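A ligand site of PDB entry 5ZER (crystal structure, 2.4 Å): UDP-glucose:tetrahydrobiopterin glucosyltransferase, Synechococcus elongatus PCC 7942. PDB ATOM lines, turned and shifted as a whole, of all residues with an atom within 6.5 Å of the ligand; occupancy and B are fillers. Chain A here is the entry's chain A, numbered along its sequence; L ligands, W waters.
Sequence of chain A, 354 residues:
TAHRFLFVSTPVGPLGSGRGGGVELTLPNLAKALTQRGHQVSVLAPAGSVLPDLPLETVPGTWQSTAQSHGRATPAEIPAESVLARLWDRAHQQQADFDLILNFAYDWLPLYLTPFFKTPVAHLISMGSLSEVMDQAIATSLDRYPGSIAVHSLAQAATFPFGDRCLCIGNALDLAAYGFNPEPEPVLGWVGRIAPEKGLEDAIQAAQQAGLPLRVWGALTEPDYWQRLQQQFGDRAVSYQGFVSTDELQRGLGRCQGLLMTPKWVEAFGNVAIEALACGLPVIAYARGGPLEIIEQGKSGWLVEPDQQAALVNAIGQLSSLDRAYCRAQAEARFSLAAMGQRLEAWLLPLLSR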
ATOM      1  N   SER A   9      23.953  13.451  12.598  1.00  0.00           N
ATOM      2  CA  SER A   9      24.935  12.376  12.592  1.00  0.00           C
ATOM      3  C   SER A   9      25.148  11.726  11.199  1.00  0.00           C
ATOM      4  O   SER A   9      24.564  12.124  10.197  1.00  0.00           O
ATOM      5  CB  SER A   9      24.461  11.320  13.586  1.00  0.00           C
ATOM      6  OG  SER A   9      25.440  10.365  13.846  1.00  0.00           O
ATOM      7  N   THR A  10      26.008  10.726  11.173  1.00  0.00           N
ATOM      8  CA  THR A  10      26.211   9.918   9.988  1.00  0.00           C
ATOM      9  C   THR A  10      25.032   8.978   9.624  1.00  0.00           C
ATOM     10  O   THR A  10      24.459   8.350  10.510  1.00  0.00           O
ATOM     11  CB  THR A  10      27.480   9.058  10.122  1.00  0.00           C
ATOM     12  OG1 THR A  10      27.488   8.094   9.062  1.00  0.00           O
ATOM     13  CG2 THR A  10      27.573   8.320  11.484  1.00  0.00           C
ATOM     14  N   PRO A  11      24.684   8.878   8.321  1.00  0.00           N
ATOM     15  CA  PRO A  11      23.675   7.898   7.910  1.00  0.00           C
ATOM     16  C   PRO A  11      24.191   6.488   7.672  1.00  0.00           C
ATOM     17  O   PRO A  11      23.437   5.662   7.148  1.00  0.00           O
ATOM     18  CB  PRO A  11      23.209   8.458   6.571  1.00  0.00           C
ATOM     19  CG  PRO A  11      24.462   9.024   6.007  1.00  0.00           C
ATOM     20  CD  PRO A  11      24.988   9.774   7.188  1.00  0.00           C
ATOM     21  N   VAL A  12      25.462   6.196   7.963  1.00  0.00           N
ATOM     22  CA  VAL A  12      25.954   4.837   7.707  1.00  0.00           C
ATOM     23  C   VAL A  12      25.408   3.856   8.694  1.00  0.00           C
ATOM     24  O   VAL A  12      25.173   2.702   8.334  1.00  0.00           O
ATOM     25  CB  VAL A  12      27.474   4.710   7.681  1.00  0.00           C
ATOM     26  CG1 VAL A  12      28.055   5.578   6.587  1.00  0.00           C
ATOM     27  CG2 VAL A  12      28.100   4.985   9.033  1.00  0.00           C
ATOM     28  N   ARG A  19      28.886   0.980  14.190  1.00  0.00           N
ATOM     29  CA  ARG A  19      28.767   1.137  12.725  1.00  0.00           C
ATOM     30  C   ARG A  19      29.069   2.554  12.250  1.00  0.00           C
ATOM     31  O   ARG A  19      29.617   2.735  11.149  1.00  0.00           O
ATOM     32  CB  ARG A  19      27.377   0.702  12.255  1.00  0.00           C
ATOM     33  CG  ARG A  19      27.200  -0.797  12.337  1.00  0.00           C
ATOM     34  CD  ARG A  19      25.746  -1.213  12.469  1.00  0.00           C
ATOM     35  NE  ARG A  19      25.655  -2.647  12.745  1.00  0.00           N
ATOM     36  CZ  ARG A  19      24.646  -3.259  13.370  1.00  0.00           C
ATOM     37  NH1 ARG A  19      23.585  -2.578  13.823  1.00  0.00           N
ATOM     38  NH2 ARG A  19      24.703  -4.580  13.556  1.00  0.00           N
ATOM     39  N   GLY A  20      28.725   3.543  13.088  1.00  0.00           N
ATOM     40  CA  GLY A  20      29.015   4.959  12.811  1.00  0.00           C
ATOM     41  C   GLY A  20      30.471   5.378  12.805  1.00  0.00           C
ATOM     42  O   GLY A  20      30.775   6.556  12.561  1.00  0.00           O
ATOM     43  N   GLY A  21      31.382   4.465  13.121  1.00  0.00           N
ATOM     44  CA  GLY A  21      32.804   4.731  13.065  1.00  0.00           C
ATOM     45  C   GLY A  21      33.248   5.686  14.139  1.00  0.00           C
ATOM     46  O   GLY A  21      32.771   5.608  15.273  1.00  0.00           O
ATOM     47  N   GLY A  22      34.161   6.573  13.783  1.00  0.00           N
ATOM     48  CA  GLY A  22      34.692   7.594  14.692  1.00  0.00           C
ATOM     49  C   GLY A  22      33.763   8.758  15.005  1.00  0.00           C
ATOM     50  O   GLY A  22      34.040   9.574  15.918  1.00  0.00           O
ATOM     51  N   VAL A  23      32.655   8.839  14.270  1.00  0.00           N
ATOM     52  CA  VAL A  23      31.605   9.812  14.566  1.00  0.00           C
ATOM     53  C   VAL A  23      30.962   9.435  15.908  1.00  0.00           C
ATOM     54  O   VAL A  23      30.550  10.319  16.669  1.00  0.00           O
ATOM     55  CB  VAL A  23      30.513   9.839  13.481  1.00  0.00           C
ATOM     56  CG1 VAL A  23      29.522  10.965  13.734  1.00  0.00           C
ATOM     57  CG2 VAL A  23      31.144   9.999  12.103  1.00  0.00           C
ATOM     58  N   GLU A  24      30.906   8.137  16.186  1.00  0.00           N
ATOM     59  CA  GLU A  24      30.431   7.617  17.483  1.00  0.00           C
ATOM     60  C   GLU A  24      31.155   8.151  18.683  1.00  0.00           C
ATOM     61  O   GLU A  24      30.583   8.192  19.760  1.00  0.00           O
ATOM     62  CB  GLU A  24      30.487   6.102  17.515  1.00  0.00           C
ATOM     63  CG  GLU A  24      29.597   5.495  16.450  1.00  0.00           C
ATOM     64  CD  GLU A  24      29.027   4.165  16.829  1.00  0.00           C
ATOM     65  OE1 GLU A  24      29.372   3.654  17.920  1.00  0.00           O
ATOM     66  OE2 GLU A  24      28.250   3.619  16.016  1.00  0.00           O
ATOM     67  N   THR A  26      33.292  11.220  17.973  1.00  0.00           N
ATOM     68  CA  THR A  26      33.503  12.645  17.690  1.00  0.00           C
ATOM     69  C   THR A  26      32.275  13.488  18.039  1.00  0.00           C
ATOM     70  O   THR A  26      32.408  14.571  18.636  1.00  0.00           O
ATOM     71  CB  THR A  26      33.879  12.899  16.212  1.00  0.00           C
ATOM     72  OG1 THR A  26      35.001  12.100  15.872  1.00  0.00           O
ATOM     73  CG2 THR A  26      34.243  14.359  15.967  1.00  0.00           C
ATOM     74  N   GLN A  64      23.063   4.663   4.447  1.00  0.00           N
ATOM     75  CA  GLN A  64      23.799   5.066   3.274  1.00  0.00           C
ATOM     76  C   GLN A  64      25.040   4.197   3.183  1.00  0.00           C
ATOM     77  O   GLN A  64      25.713   3.968   4.179  1.00  0.00           O
ATOM     78  CB  GLN A  64      24.148   6.556   3.358  1.00  0.00           C
ATOM     79  CG  GLN A  64      24.693   7.172   2.063  1.00  0.00           C
ATOM     80  CD  GLN A  64      23.652   7.732   1.085  1.00  0.00           C
ATOM     81  OE1 GLN A  64      22.449   7.747   1.359  1.00  0.00           O
ATOM     82  NE2 GLN A  64      24.141   8.177  -0.076  1.00  0.00           N
ATOM     83  N   SER A  65      25.343   3.731   1.972  1.00  0.00           N
ATOM     84  CA  SER A  65      26.579   2.995   1.688  1.00  0.00           C
ATOM     85  C   SER A  65      27.845   3.798   2.038  1.00  0.00           C
ATOM     86  O   SER A  65      27.931   4.983   1.733  1.00  0.00           O
ATOM     87  CB  SER A  65      26.634   2.610   0.212  1.00  0.00           C
ATOM     88  OG  SER A  65      26.329   3.732  -0.598  1.00  0.00           O
ATOM     89  N   THR A  66      28.804   3.143   2.690  1.00  0.00           N
ATOM     90  CA  THR A  66      30.053   3.799   3.044  1.00  0.00           C
ATOM     91  C   THR A  66      30.718   4.313   1.762  1.00  0.00           C
ATOM     92  O   THR A  66      30.779   3.588   0.748  1.00  0.00           O
ATOM     93  CB  THR A  66      31.003   2.886   3.892  1.00  0.00           C
ATOM     94  OG1 THR A  66      32.135   3.639   4.364  1.00  0.00           O
ATOM     95  CG2 THR A  66      31.502   1.676   3.111  1.00  0.00           C
ATOM     96  N   ALA A  67      31.173   5.572   1.817  1.00  0.00           N
ATOM     97  CA  ALA A  67      31.758   6.255   0.667  1.00  0.00           C
ATOM     98  C   ALA A  67      33.078   5.624   0.183  1.00  0.00           C
ATOM     99  O   ALA A  67      33.347   5.596  -1.026  1.00  0.00           O
ATOM    100  CB  ALA A  67      31.979   7.723   0.984  1.00  0.00           C
ATOM    101  N   GLN A  68      33.897   5.122   1.106  1.00  0.00           N
ATOM    102  CA  GLN A  68      35.197   4.479   0.756  1.00  0.00           C
ATOM    103  C   GLN A  68      35.074   3.232  -0.139  1.00  0.00           C
ATOM    104  O   GLN A  68      36.011   2.921  -0.888  1.00  0.00           O
ATOM    105  CB  GLN A  68      36.028   4.171   2.017  1.00  0.00           C
ATOM    106  CG  GLN A  68      35.382   3.221   3.032  1.00  0.00           C
ATOM    107  CD  GLN A  68      35.579   3.675   4.466  1.00  0.00           C
ATOM    108  OE1 GLN A  68      36.696   3.985   4.894  1.00  0.00           O
ATOM    109  NE2 GLN A  68      34.488   3.693   5.235  1.00  0.00           N
ATOM    110  N   PHE A 104      27.659  16.043  10.203  1.00  0.00           N
ATOM    111  CA  PHE A 104      28.786  15.066  10.301  1.00  0.00           C
ATOM    112  C   PHE A 104      28.882  14.043   9.183  1.00  0.00           C
ATOM    113  O   PHE A 104      29.763  13.176   9.207  1.00  0.00           O
ATOM    114  CB  PHE A 104      28.675  14.291  11.629  1.00  0.00           C
ATOM    115  CG  PHE A 104      28.878  15.126  12.819  1.00  0.00           C
ATOM    116  CD1 PHE A 104      27.927  16.114  13.165  1.00  0.00           C
ATOM    117  CD2 PHE A 104      29.984  14.967  13.600  1.00  0.00           C
ATOM    118  CE1 PHE A 104      28.088  16.900  14.280  1.00  0.00           C
ATOM    119  CE2 PHE A 104      30.156  15.766  14.720  1.00  0.00           C
ATOM    120  CZ  PHE A 104      29.213  16.730  15.067  1.00  0.00           C
ATOM    121  N   ALA A 105      27.966  14.094   8.221  1.00  0.00           N
ATOM    122  CA  ALA A 105      27.916  13.074   7.172  1.00  0.00           C
ATOM    123  C   ALA A 105      28.829  13.441   6.019  1.00  0.00           C
ATOM    124  O   ALA A 105      28.829  14.581   5.556  1.00  0.00           O
ATOM    125  CB  ALA A 105      26.495  12.882   6.653  1.00  0.00           C
ATOM    126  N   TYR A 106      29.593  12.442   5.589  1.00  0.00           N
ATOM    127  CA  TYR A 106      30.415  12.516   4.410  1.00  0.00           C
ATOM    128  C   TYR A 106      29.587  12.142   3.220  1.00  0.00           C
ATOM    129  O   TYR A 106      29.731  11.040   2.679  1.00  0.00           O
ATOM    130  CB  TYR A 106      31.605  11.560   4.519  1.00  0.00           C
ATOM    131  CG  TYR A 106      32.664  11.839   3.452  1.00  0.00           C
ATOM    132  CD1 TYR A 106      33.564  12.878   3.597  1.00  0.00           C
ATOM    133  CD2 TYR A 106      32.749  11.068   2.303  1.00  0.00           C
ATOM    134  CE1 TYR A 106      34.524  13.129   2.639  1.00  0.00           C
ATOM    135  CE2 TYR A 106      33.708  11.314   1.336  1.00  0.00           C
ATOM    136  CZ  TYR A 106      34.605  12.333   1.505  1.00  0.00           C
ATOM    137  OH  TYR A 106      35.577  12.580   0.502  1.00  0.00           O
ATOM    138  N   ASP A 107      28.736  13.068   2.781  1.00  0.00           N
ATOM    139  CA  ASP A 107      27.854  12.790   1.663  1.00  0.00           C
ATOM    140  C   ASP A 107      27.524  14.072   0.900  1.00  0.00           C
ATOM    141  O   ASP A 107      27.601  15.173   1.452  1.00  0.00           O
ATOM    142  CB  ASP A 107      26.565  12.134   2.164  1.00  0.00           C
ATOM    143  CG  ASP A 107      26.785  10.684   2.609  1.00  0.00           C
ATOM    144  OD1 ASP A 107      26.776  10.433   3.841  1.00  0.00           O
ATOM    145  OD2 ASP A 107      26.995   9.824   1.719  1.00  0.00           O
ATOM    146  N   SER A 126      35.015  14.178   7.402  1.00  0.00           N
ATOM    147  CA  SER A 126      35.644  13.178   8.244  1.00  0.00           C
ATOM    148  C   SER A 126      36.611  12.249   7.541  1.00  0.00           C
ATOM    149  O   SER A 126      37.285  11.478   8.204  1.00  0.00           O
ATOM    150  CB  SER A 126      34.540  12.367   8.903  1.00  0.00           C
ATOM    151  OG  SER A 126      33.807  11.614   7.967  1.00  0.00           O
ATOM    152  N   MET A 127      36.683  12.285   6.214  1.00  0.00           N
ATOM    153  CA  MET A 127      37.632  11.432   5.456  1.00  0.00           C
ATOM    154  C   MET A 127      38.279  12.261   4.372  1.00  0.00           C
ATOM    155  O   MET A 127      37.953  13.446   4.208  1.00  0.00           O
ATOM    156  CB  MET A 127      36.869  10.232   4.906  1.00  0.00           C
ATOM    157  CG  MET A 127      36.489   9.280   6.025  1.00  0.00           C
ATOM    158  SD  MET A 127      35.477   7.803   5.255  1.00  0.00           S
ATOM    159  CE  MET A 127      33.908   8.793   4.631  1.00  0.00           C
HETATM  160  N1  LIG L   1      30.179   7.108   4.283  1.00  0.00           N
HETATM  161  N2  LIG L   1      28.612   7.920   2.768  1.00  0.00           N
HETATM  162  C1  LIG L   1      29.184   8.000   3.991  1.00  0.00           C
HETATM  163  N3  LIG L   1      28.779   8.927   4.889  1.00  0.00           N
HETATM  164  C2  LIG L   1      29.327   9.058   6.093  1.00  0.00           C
HETATM  165  O1  LIG L   1      28.943   9.946   6.909  1.00  0.00           O
HETATM  166  C3  LIG L   1      30.393   8.117   6.459  1.00  0.00           C
HETATM  167  C4  LIG L   1      30.805   7.116   5.477  1.00  0.00           C
HETATM  168  N4  LIG L   1      31.759   6.225   5.780  1.00  0.00           N
HETATM  169  C5  LIG L   1      32.438   6.221   7.085  1.00  0.00           C
HETATM  170  C6  LIG L   1      31.957   7.312   8.027  1.00  0.00           C
HETATM  171  N5  LIG L   1      30.972   8.163   7.666  1.00  0.00           N
HETATM  172  C7  LIG L   1      32.498   7.468   9.414  1.00  0.00           C
HETATM  173  O2  LIG L   1      32.584   6.178  10.021  1.00  0.00           O
HETATM  174  C8  LIG L   1      33.874   8.046   9.523  1.00  0.00           C
HETATM  175  O3  LIG L   1      34.040   9.033   8.513  1.00  0.00           O
HETATM  176  C9  LIG L   1      34.033   8.668  10.896  1.00  0.00           C
HETATM  177  O   HOH W   1      35.173  10.868  12.541  1.00  0.00           O
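N of Gly 20 sits at hydrogen-bond distance from OE2 of Glu 24 (3.0 Å). OG1 of Thr 26 lies within hydrogen-bond range of O of Gly 22 (2.7 Å). The side-chain hydroxyl (OG1) of Thr 66 lies within hydrogen-bond range of the side-chain amide nitrogen (NE2) of Gln 68. The backbone NH (N) of Val 12 sits at hydrogen-bond distance from the side-chain hydroxyl (OG1) of Thr 10 (3.0 Å). N of Gln 64 is in hydrogen-bond range of O of Pro 11.
Residues that only touch the ligand: Pro 11 (3.97 Å), Val 12 (3.3 Å), Gly 21 (3.4 Å), Gly 22 (3.6 Å), Val 23 (3.4 Å), Gln 68 (3.7 Å) and Ala 105 (3.3 Å). Hydrophobic or aromatic side chains that line the ligand: Pro 11, Val 12, Val 23, Ala 67, Ala 105, Tyr 106 and Met 127. Along chain A the residues within 4 Å of the ligand span positions 10 to 127. The nearest printed residue that does not touch the ligand is Phe 104 (4.05 Å).
The side-chain hydroxyl (OG1) of Thr 66 sits at hydrogen-bond distance from a nitrogen (N4) of the ligand (3.0 Å). The backbone NH (N) of Tyr 106 is in hydrogen-bond range of an oxygen (O1) of the ligand. N1 of the ligand sits at hydrogen-bond distance from N of Ala 67 (3.1 Å). OD2 of Asp 107 sits at hydrogen-bond distance from N2 of the ligand, 2.7 Å away. An oxygen (O3) of the ligand is in hydrogen-bond range of the side-chain hydroxyl (OG) of Ser 126 (2.6 Å). A nitrogen (N3) of the ligand lies within hydrogen-bond range of the backbone carbonyl oxygen (O) of Tyr 106 (3.2 Å). SD of Met 127 sits close to O3 of the ligand, 3.8 Å away. O of Ser 65 lies within hydrogen-bond range of N2 of the ligand (3.2 Å). An oxygen (O1) of the ligand is in hydrogen-bond range of the side-chain hydroxyl of Thr 10 (3.2 Å). The backbone carbonyl oxygen (O) of Gly 20 is in hydrogen-bond range of an oxygen (O2) of the ligand (3.1 Å).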
